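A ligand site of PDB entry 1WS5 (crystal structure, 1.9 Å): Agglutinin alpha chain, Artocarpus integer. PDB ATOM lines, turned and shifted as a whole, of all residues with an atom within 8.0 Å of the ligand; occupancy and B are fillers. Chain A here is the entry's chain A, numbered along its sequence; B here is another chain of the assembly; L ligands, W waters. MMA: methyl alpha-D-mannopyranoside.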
ATOM      1  N   GLY A   1     -23.441  32.181   3.180  1.00  0.00           N
ATOM      2  CA  GLY A   1     -22.149  32.121   3.935  1.00  0.00           C
ATOM      3  C   GLY A   1     -21.646  33.494   4.302  1.00  0.00           C
ATOM      4  O   GLY A   1     -22.394  34.480   4.267  1.00  0.00           O
ATOM      5  N   LYS A   2     -20.369  33.584   4.670  1.00  0.00           N
ATOM      6  CA  LYS A   2     -19.779  34.851   5.045  1.00  0.00           C
ATOM      7  C   LYS A   2     -19.123  35.509   3.833  1.00  0.00           C
ATOM      8  O   LYS A   2     -18.230  34.945   3.202  1.00  0.00           O
ATOM      9  CB  LYS A   2     -18.720  34.652   6.131  1.00  0.00           C
ATOM     10  CG  LYS A   2     -18.137  35.958   6.651  1.00  0.00           C
ATOM     11  CD  LYS A   2     -17.099  35.708   7.724  1.00  0.00           C
ATOM     12  CE  LYS A   2     -16.508  37.025   8.218  1.00  0.00           C
ATOM     13  NZ  LYS A   2     -15.458  36.802   9.250  1.00  0.00           N
ATOM     14  N   ALA A  24     -17.378  20.412  -3.372  1.00  0.00           N
ATOM     15  CA  ALA A  24     -17.071  21.693  -3.999  1.00  0.00           C
ATOM     16  C   ALA A  24     -15.846  22.375  -3.413  1.00  0.00           C
ATOM     17  O   ALA A  24     -15.114  21.789  -2.622  1.00  0.00           O
ATOM     18  CB  ALA A  24     -18.278  22.622  -3.880  1.00  0.00           C
ATOM     19  N   ILE A  25     -15.630  23.614  -3.833  1.00  0.00           N
ATOM     20  CA  ILE A  25     -14.507  24.399  -3.356  1.00  0.00           C
ATOM     21  C   ILE A  25     -14.778  24.919  -1.941  1.00  0.00           C
ATOM     22  O   ILE A  25     -15.891  25.335  -1.613  1.00  0.00           O
ATOM     23  CB  ILE A  25     -14.244  25.574  -4.321  1.00  0.00           C
ATOM     24  CG1 ILE A  25     -13.761  24.998  -5.650  1.00  0.00           C
ATOM     25  CG2 ILE A  25     -13.235  26.549  -3.729  1.00  0.00           C
ATOM     26  CD1 ILE A  25     -13.698  25.976  -6.734  1.00  0.00           C
ATOM     27  N   SER A  46     -13.736  27.841   4.902  1.00  0.00           N
ATOM     28  CA  SER A  46     -15.002  27.145   4.957  1.00  0.00           C
ATOM     29  C   SER A  46     -15.327  26.904   6.428  1.00  0.00           C
ATOM     30  O   SER A  46     -14.413  26.906   7.259  1.00  0.00           O
ATOM     31  CB  SER A  46     -14.888  25.793   4.253  1.00  0.00           C
ATOM     32  OG  SER A  46     -15.910  24.907   4.685  1.00  0.00           O
ATOM     33  N   PHE A  47     -16.596  26.697   6.757  1.00  0.00           N
ATOM     34  CA  PHE A  47     -16.970  26.443   8.135  1.00  0.00           C
ATOM     35  C   PHE A  47     -16.747  24.974   8.502  1.00  0.00           C
ATOM     36  O   PHE A  47     -16.841  24.596   9.664  1.00  0.00           O
ATOM     37  CB  PHE A  47     -18.437  26.814   8.386  1.00  0.00           C
ATOM     38  CG  PHE A  47     -18.727  28.277   8.229  1.00  0.00           C
ATOM     39  CD1 PHE A  47     -17.823  29.241   8.675  1.00  0.00           C
ATOM     40  CD2 PHE A  47     -19.919  28.699   7.652  1.00  0.00           C
ATOM     41  CE1 PHE A  47     -18.109  30.609   8.551  1.00  0.00           C
ATOM     42  CE2 PHE A  47     -20.211  30.063   7.521  1.00  0.00           C
ATOM     43  CZ  PHE A  47     -19.304  31.009   7.974  1.00  0.00           C
ATOM     44  N   ILE A  48     -16.460  24.151   7.498  1.00  0.00           N
ATOM     45  CA  ILE A  48     -16.231  22.730   7.746  1.00  0.00           C
ATOM     46  C   ILE A  48     -14.834  22.330   7.268  1.00  0.00           C
ATOM     47  O   ILE A  48     -14.122  23.138   6.693  1.00  0.00           O
ATOM     48  CB  ILE A  48     -17.298  21.839   7.058  1.00  0.00           C
ATOM     49  CG1 ILE A  48     -17.269  22.067   5.542  1.00  0.00           C
ATOM     50  CG2 ILE A  48     -18.668  22.170   7.621  1.00  0.00           C
ATOM     51  CD1 ILE A  48     -18.272  21.207   4.780  1.00  0.00           C
ATOM     52  N   VAL A  75     -25.072  21.307  -4.090  1.00  0.00           N
ATOM     53  CA  VAL A  75     -24.394  20.447  -3.129  1.00  0.00           C
ATOM     54  C   VAL A  75     -25.505  20.544  -2.091  1.00  0.00           C
ATOM     55  O   VAL A  75     -25.705  21.602  -1.484  1.00  0.00           O
ATOM     56  CB  VAL A  75     -23.103  21.046  -2.601  1.00  0.00           C
ATOM     57  CG1 VAL A  75     -22.576  20.175  -1.469  1.00  0.00           C
ATOM     58  CG2 VAL A  75     -22.070  21.114  -3.717  1.00  0.00           C
ATOM     59  N   SER A  76     -26.252  19.456  -1.928  1.00  0.00           N
ATOM     60  CA  SER A  76     -27.414  19.478  -1.050  1.00  0.00           C
ATOM     61  C   SER A  76     -28.316  20.528  -1.708  1.00  0.00           C
ATOM     62  O   SER A  76     -28.457  20.526  -2.917  1.00  0.00           O
ATOM     63  CB  SER A  76     -27.039  19.843   0.375  1.00  0.00           C
ATOM     64  OG  SER A  76     -26.429  18.740   1.021  1.00  0.00           O
ATOM     65  N   GLY A  77     -28.897  21.433  -0.935  1.00  0.00           N
ATOM     66  CA  GLY A  77     -29.776  22.415  -1.577  1.00  0.00           C
ATOM     67  C   GLY A  77     -29.102  23.687  -2.080  1.00  0.00           C
ATOM     68  O   GLY A  77     -29.709  24.467  -2.814  1.00  0.00           O
ATOM     69  N   TYR A  78     -27.849  23.886  -1.707  1.00  0.00           N
ATOM     70  CA  TYR A  78     -27.131  25.102  -2.073  1.00  0.00           C
ATOM     71  C   TYR A  78     -26.426  25.104  -3.423  1.00  0.00           C
ATOM     72  O   TYR A  78     -25.747  24.150  -3.778  1.00  0.00           O
ATOM     73  CB  TYR A  78     -26.090  25.398  -0.979  1.00  0.00           C
ATOM     74  CG  TYR A  78     -26.716  25.532   0.385  1.00  0.00           C
ATOM     75  CD1 TYR A  78     -27.306  26.728   0.790  1.00  0.00           C
ATOM     76  CD2 TYR A  78     -26.751  24.445   1.256  1.00  0.00           C
ATOM     77  CE1 TYR A  78     -27.929  26.843   2.032  1.00  0.00           C
ATOM     78  CE2 TYR A  78     -27.381  24.553   2.508  1.00  0.00           C
ATOM     79  CZ  TYR A  78     -27.968  25.746   2.883  1.00  0.00           C
ATOM     80  OH  TYR A  78     -28.582  25.854   4.105  1.00  0.00           O
ATOM     81  N   VAL A  79     -26.592  26.196  -4.173  1.00  0.00           N
ATOM     82  CA  VAL A  79     -25.912  26.332  -5.458  1.00  0.00           C
ATOM     83  C   VAL A  79     -24.561  26.932  -5.101  1.00  0.00           C
ATOM     84  O   VAL A  79     -24.490  28.000  -4.497  1.00  0.00           O
ATOM     85  CB  VAL A  79     -26.654  27.286  -6.412  1.00  0.00           C
ATOM     86  CG1 VAL A  79     -25.822  27.505  -7.675  1.00  0.00           C
ATOM     87  CG2 VAL A  79     -28.012  26.696  -6.797  1.00  0.00           C
ATOM     88  N   VAL A  80     -23.492  26.245  -5.460  1.00  0.00           N
ATOM     89  CA  VAL A  80     -22.148  26.716  -5.143  1.00  0.00           C
ATOM     90  C   VAL A  80     -21.193  26.509  -6.315  1.00  0.00           C
ATOM     91  O   VAL A  80     -21.579  25.994  -7.371  1.00  0.00           O
ATOM     92  CB  VAL A  80     -21.578  25.955  -3.920  1.00  0.00           C
ATOM     93  CG1 VAL A  80     -22.450  26.204  -2.702  1.00  0.00           C
ATOM     94  CG2 VAL A  80     -21.495  24.468  -4.217  1.00  0.00           C
ATOM     95  N   VAL A  81     -19.948  26.924  -6.124  1.00  0.00           N
ATOM     96  CA  VAL A  81     -18.928  26.757  -7.144  1.00  0.00           C
ATOM     97  C   VAL A  81     -18.295  25.403  -6.862  1.00  0.00           C
ATOM     98  O   VAL A  81     -17.552  25.246  -5.892  1.00  0.00           O
ATOM     99  CB  VAL A  81     -17.847  27.865  -7.053  1.00  0.00           C
ATOM    100  CG1 VAL A  81     -16.796  27.650  -8.118  1.00  0.00           C
ATOM    101  CG2 VAL A  81     -18.501  29.224  -7.217  1.00  0.00           C
ATOM    102  N   SER A 119     -18.293  34.847  -1.340  1.00  0.00           N
ATOM    103  CA  SER A 119     -18.892  34.422  -0.086  1.00  0.00           C
ATOM    104  C   SER A 119     -18.603  32.948   0.121  1.00  0.00           C
ATOM    105  O   SER A 119     -18.646  32.155  -0.818  1.00  0.00           O
ATOM    106  CB  SER A 119     -20.402  34.656  -0.115  1.00  0.00           C
ATOM    107  OG  SER A 119     -21.011  34.138   1.052  1.00  0.00           O
ATOM    108  N   ILE A 120     -18.314  32.574   1.357  1.00  0.00           N
ATOM    109  CA  ILE A 120     -18.029  31.187   1.667  1.00  0.00           C
ATOM    110  C   ILE A 120     -18.711  30.769   2.961  1.00  0.00           C
ATOM    111  O   ILE A 120     -18.597  31.448   3.971  1.00  0.00           O
ATOM    112  CB  ILE A 120     -16.505  30.947   1.831  1.00  0.00           C
ATOM    113  CG1 ILE A 120     -15.774  31.278   0.524  1.00  0.00           C
ATOM    114  CG2 ILE A 120     -16.247  29.502   2.268  1.00  0.00           C
ATOM    115  CD1 ILE A 120     -14.260  31.182   0.619  1.00  0.00           C
ATOM    116  N   GLY A 121     -19.435  29.654   2.900  1.00  0.00           N
ATOM    117  CA  GLY A 121     -20.103  29.096   4.069  1.00  0.00           C
ATOM    118  C   GLY A 121     -19.428  27.751   4.206  1.00  0.00           C
ATOM    119  O   GLY A 121     -18.262  27.670   4.593  1.00  0.00           O
ATOM    120  N   TYR A 122     -20.143  26.677   3.882  1.00  0.00           N
ATOM    121  CA  TYR A 122     -19.544  25.354   3.917  1.00  0.00           C
ATOM    122  C   TYR A 122     -18.675  25.276   2.665  1.00  0.00           C
ATOM    123  O   TYR A 122     -17.608  24.655   2.664  1.00  0.00           O
ATOM    124  CB  TYR A 122     -20.622  24.260   3.858  1.00  0.00           C
ATOM    125  CG  TYR A 122     -21.190  23.870   5.209  1.00  0.00           C
ATOM    126  CD1 TYR A 122     -21.171  24.773   6.284  1.00  0.00           C
ATOM    127  CD2 TYR A 122     -21.757  22.616   5.416  1.00  0.00           C
ATOM    128  CE1 TYR A 122     -21.695  24.421   7.531  1.00  0.00           C
ATOM    129  CE2 TYR A 122     -22.286  22.251   6.660  1.00  0.00           C
ATOM    130  CZ  TYR A 122     -22.252  23.155   7.706  1.00  0.00           C
ATOM    131  OH  TYR A 122     -22.769  22.814   8.926  1.00  0.00           O
ATOM    132  N   TRP A 123     -19.137  25.925   1.610  1.00  0.00           N
ATOM    133  CA  TRP A 123     -18.425  25.947   0.329  1.00  0.00           C
ATOM    134  C   TRP A 123     -18.466  27.346  -0.280  1.00  0.00           C
ATOM    135  O   TRP A 123     -19.170  28.224   0.212  1.00  0.00           O
ATOM    136  CB  TRP A 123     -19.081  24.952  -0.644  1.00  0.00           C
ATOM    137  CG  TRP A 123     -19.205  23.572  -0.071  1.00  0.00           C
ATOM    138  CD1 TRP A 123     -18.195  22.684   0.140  1.00  0.00           C
ATOM    139  CD2 TRP A 123     -20.385  22.978   0.476  1.00  0.00           C
ATOM    140  NE1 TRP A 123     -18.672  21.570   0.800  1.00  0.00           N
ATOM    141  CE2 TRP A 123     -20.018  21.723   1.017  1.00  0.00           C
ATOM    142  CE3 TRP A 123     -21.726  23.383   0.565  1.00  0.00           C
ATOM    143  CZ2 TRP A 123     -20.934  20.876   1.637  1.00  0.00           C
ATOM    144  CZ3 TRP A 123     -22.641  22.527   1.190  1.00  0.00           C
ATOM    145  CH2 TRP A 123     -22.241  21.293   1.718  1.00  0.00           C
ATOM    146  N   LEU A 124     -17.701  27.554  -1.346  1.00  0.00           N
ATOM    147  CA  LEU A 124     -17.664  28.836  -2.020  1.00  0.00           C
ATOM    148  C   LEU A 124     -19.032  29.040  -2.698  1.00  0.00           C
ATOM    149  O   LEU A 124     -19.341  28.373  -3.697  1.00  0.00           O
ATOM    150  CB  LEU A 124     -16.547  28.847  -3.064  1.00  0.00           C
ATOM    151  CG  LEU A 124     -16.348  30.082  -3.946  1.00  0.00           C
ATOM    152  CD1 LEU A 124     -16.087  31.315  -3.094  1.00  0.00           C
ATOM    153  CD2 LEU A 124     -15.190  29.831  -4.898  1.00  0.00           C
ATOM    154  N   ASP A 125     -19.842  29.940  -2.150  1.00  0.00           N
ATOM    155  CA  ASP A 125     -21.179  30.216  -2.692  1.00  0.00           C
ATOM    156  C   ASP A 125     -21.140  30.886  -4.052  1.00  0.00           C
ATOM    157  O   ASP A 125     -21.870  30.506  -4.974  1.00  0.00           O
ATOM    158  CB  ASP A 125     -21.962  31.111  -1.731  1.00  0.00           C
ATOM    159  CG  ASP A 125     -22.208  30.450  -0.392  1.00  0.00           C
ATOM    160  OD1 ASP A 125     -22.749  29.332  -0.385  1.00  0.00           O
ATOM    161  OD2 ASP A 125     -21.870  31.059   0.643  1.00  0.00           O
ATOM    162  N   TYR A 126     -20.308  31.915  -4.173  1.00  0.00           N
ATOM    163  CA  TYR A 126     -20.186  32.657  -5.413  1.00  0.00           C
ATOM    164  C   TYR A 126     -18.948  33.533  -5.323  1.00  0.00           C
ATOM    165  O   TYR A 126     -18.394  33.737  -4.248  1.00  0.00           O
ATOM    166  CB  TYR A 126     -21.427  33.517  -5.647  1.00  0.00           C
ATOM    167  CG  TYR A 126     -21.679  34.546  -4.556  1.00  0.00           C
ATOM    168  CD1 TYR A 126     -20.930  35.726  -4.480  1.00  0.00           C
ATOM    169  CD2 TYR A 126     -22.667  34.332  -3.590  1.00  0.00           C
ATOM    170  CE1 TYR A 126     -21.156  36.661  -3.462  1.00  0.00           C
ATOM    171  CE2 TYR A 126     -22.899  35.263  -2.580  1.00  0.00           C
ATOM    172  CZ  TYR A 126     -22.145  36.414  -2.522  1.00  0.00           C
ATOM    173  OH  TYR A 126     -22.389  37.338  -1.525  1.00  0.00           O
ATOM    174  N   ALA B  17     -24.159  31.041  -6.598  1.00  0.00           N
ATOM    175  CA  ALA B  17     -25.504  31.320  -6.087  1.00  0.00           C
ATOM    176  C   ALA B  17     -25.942  32.737  -6.434  1.00  0.00           C
ATOM    177  O   ALA B  17     -25.126  33.645  -6.576  1.00  0.00           O
ATOM    178  CB  ALA B  17     -25.550  31.117  -4.583  1.00  0.00           C
HETATM  179  C1  MMA L   1     -23.962  26.844   5.018  1.00  0.00           C
HETATM  180  C2  MMA L   1     -24.299  28.352   5.184  1.00  0.00           C
HETATM  181  C3  MMA L   1     -25.014  28.897   3.934  1.00  0.00           C
HETATM  182  C4  MMA L   1     -24.148  28.648   2.691  1.00  0.00           C
HETATM  183  C5  MMA L   1     -23.878  27.144   2.554  1.00  0.00           C
HETATM  184  C6  MMA L   1     -22.998  26.834   1.346  1.00  0.00           C
HETATM  185  C7  MMA L   1     -25.558  24.715   5.482  1.00  0.00           C
HETATM  186  O1  MMA L   1     -25.088  26.092   5.282  1.00  0.00           O
HETATM  187  O2  MMA L   1     -23.133  29.129   5.422  1.00  0.00           O
HETATM  188  O3  MMA L   1     -25.297  30.282   4.103  1.00  0.00           O
HETATM  189  O4  MMA L   1     -24.797  29.144   1.539  1.00  0.00           O
HETATM  190  O5  MMA L   1     -23.213  26.660   3.758  1.00  0.00           O
HETATM  191  O6  MMA L   1     -21.699  27.395   1.452  1.00  0.00           O
HETATM  192  O   HOH W   1     -27.162  30.862   1.417  1.00  0.00           O
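O3 of the ligand sits at hydrogen-bond distance from N of Gly 1 (2.8 Å). An oxygen (O4) of the ligand sits at hydrogen-bond distance from the side-chain carboxylate of Asp 125 (2.8 Å). N of Trp 123 sits at hydrogen-bond distance from O6 of the ligand (3.0 Å). An oxygen (O6) of the ligand lies within hydrogen-bond range of the backbone carbonyl oxygen (O) of Trp 123 (2.9 Å). N of Tyr 122 is in hydrogen-bond range of O6 of the ligand (3.0 Å).
Merely in contact with the ligand: Phe 47, Tyr 78 and Gly 121. Seven residues have an atom within 4 Å of the ligand: Gly 1, Phe 47, Tyr 78, Gly 121, Tyr 122, Trp 123 and Asp 125. Along chain A the residues within 4 Å of the ligand span positions 1 to 125.
N of Gly 1 is in hydrogen-bond range of OD2 of Asp 125, 3.2 Å away. N of Asp 125 lies within hydrogen-bond range of O of Ser 119, at 2.8 Å. O of Asp 125 is in hydrogen-bond range of N of Ala 17 of chain B (2.9 Å). The side-chain hydroxyl of Ser 46 is in hydrogen-bond range of the backbone carbonyl oxygen of Tyr 122. O of Gly 121 lies within hydrogen-bond range of N of Phe 47 (2.9 Å).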
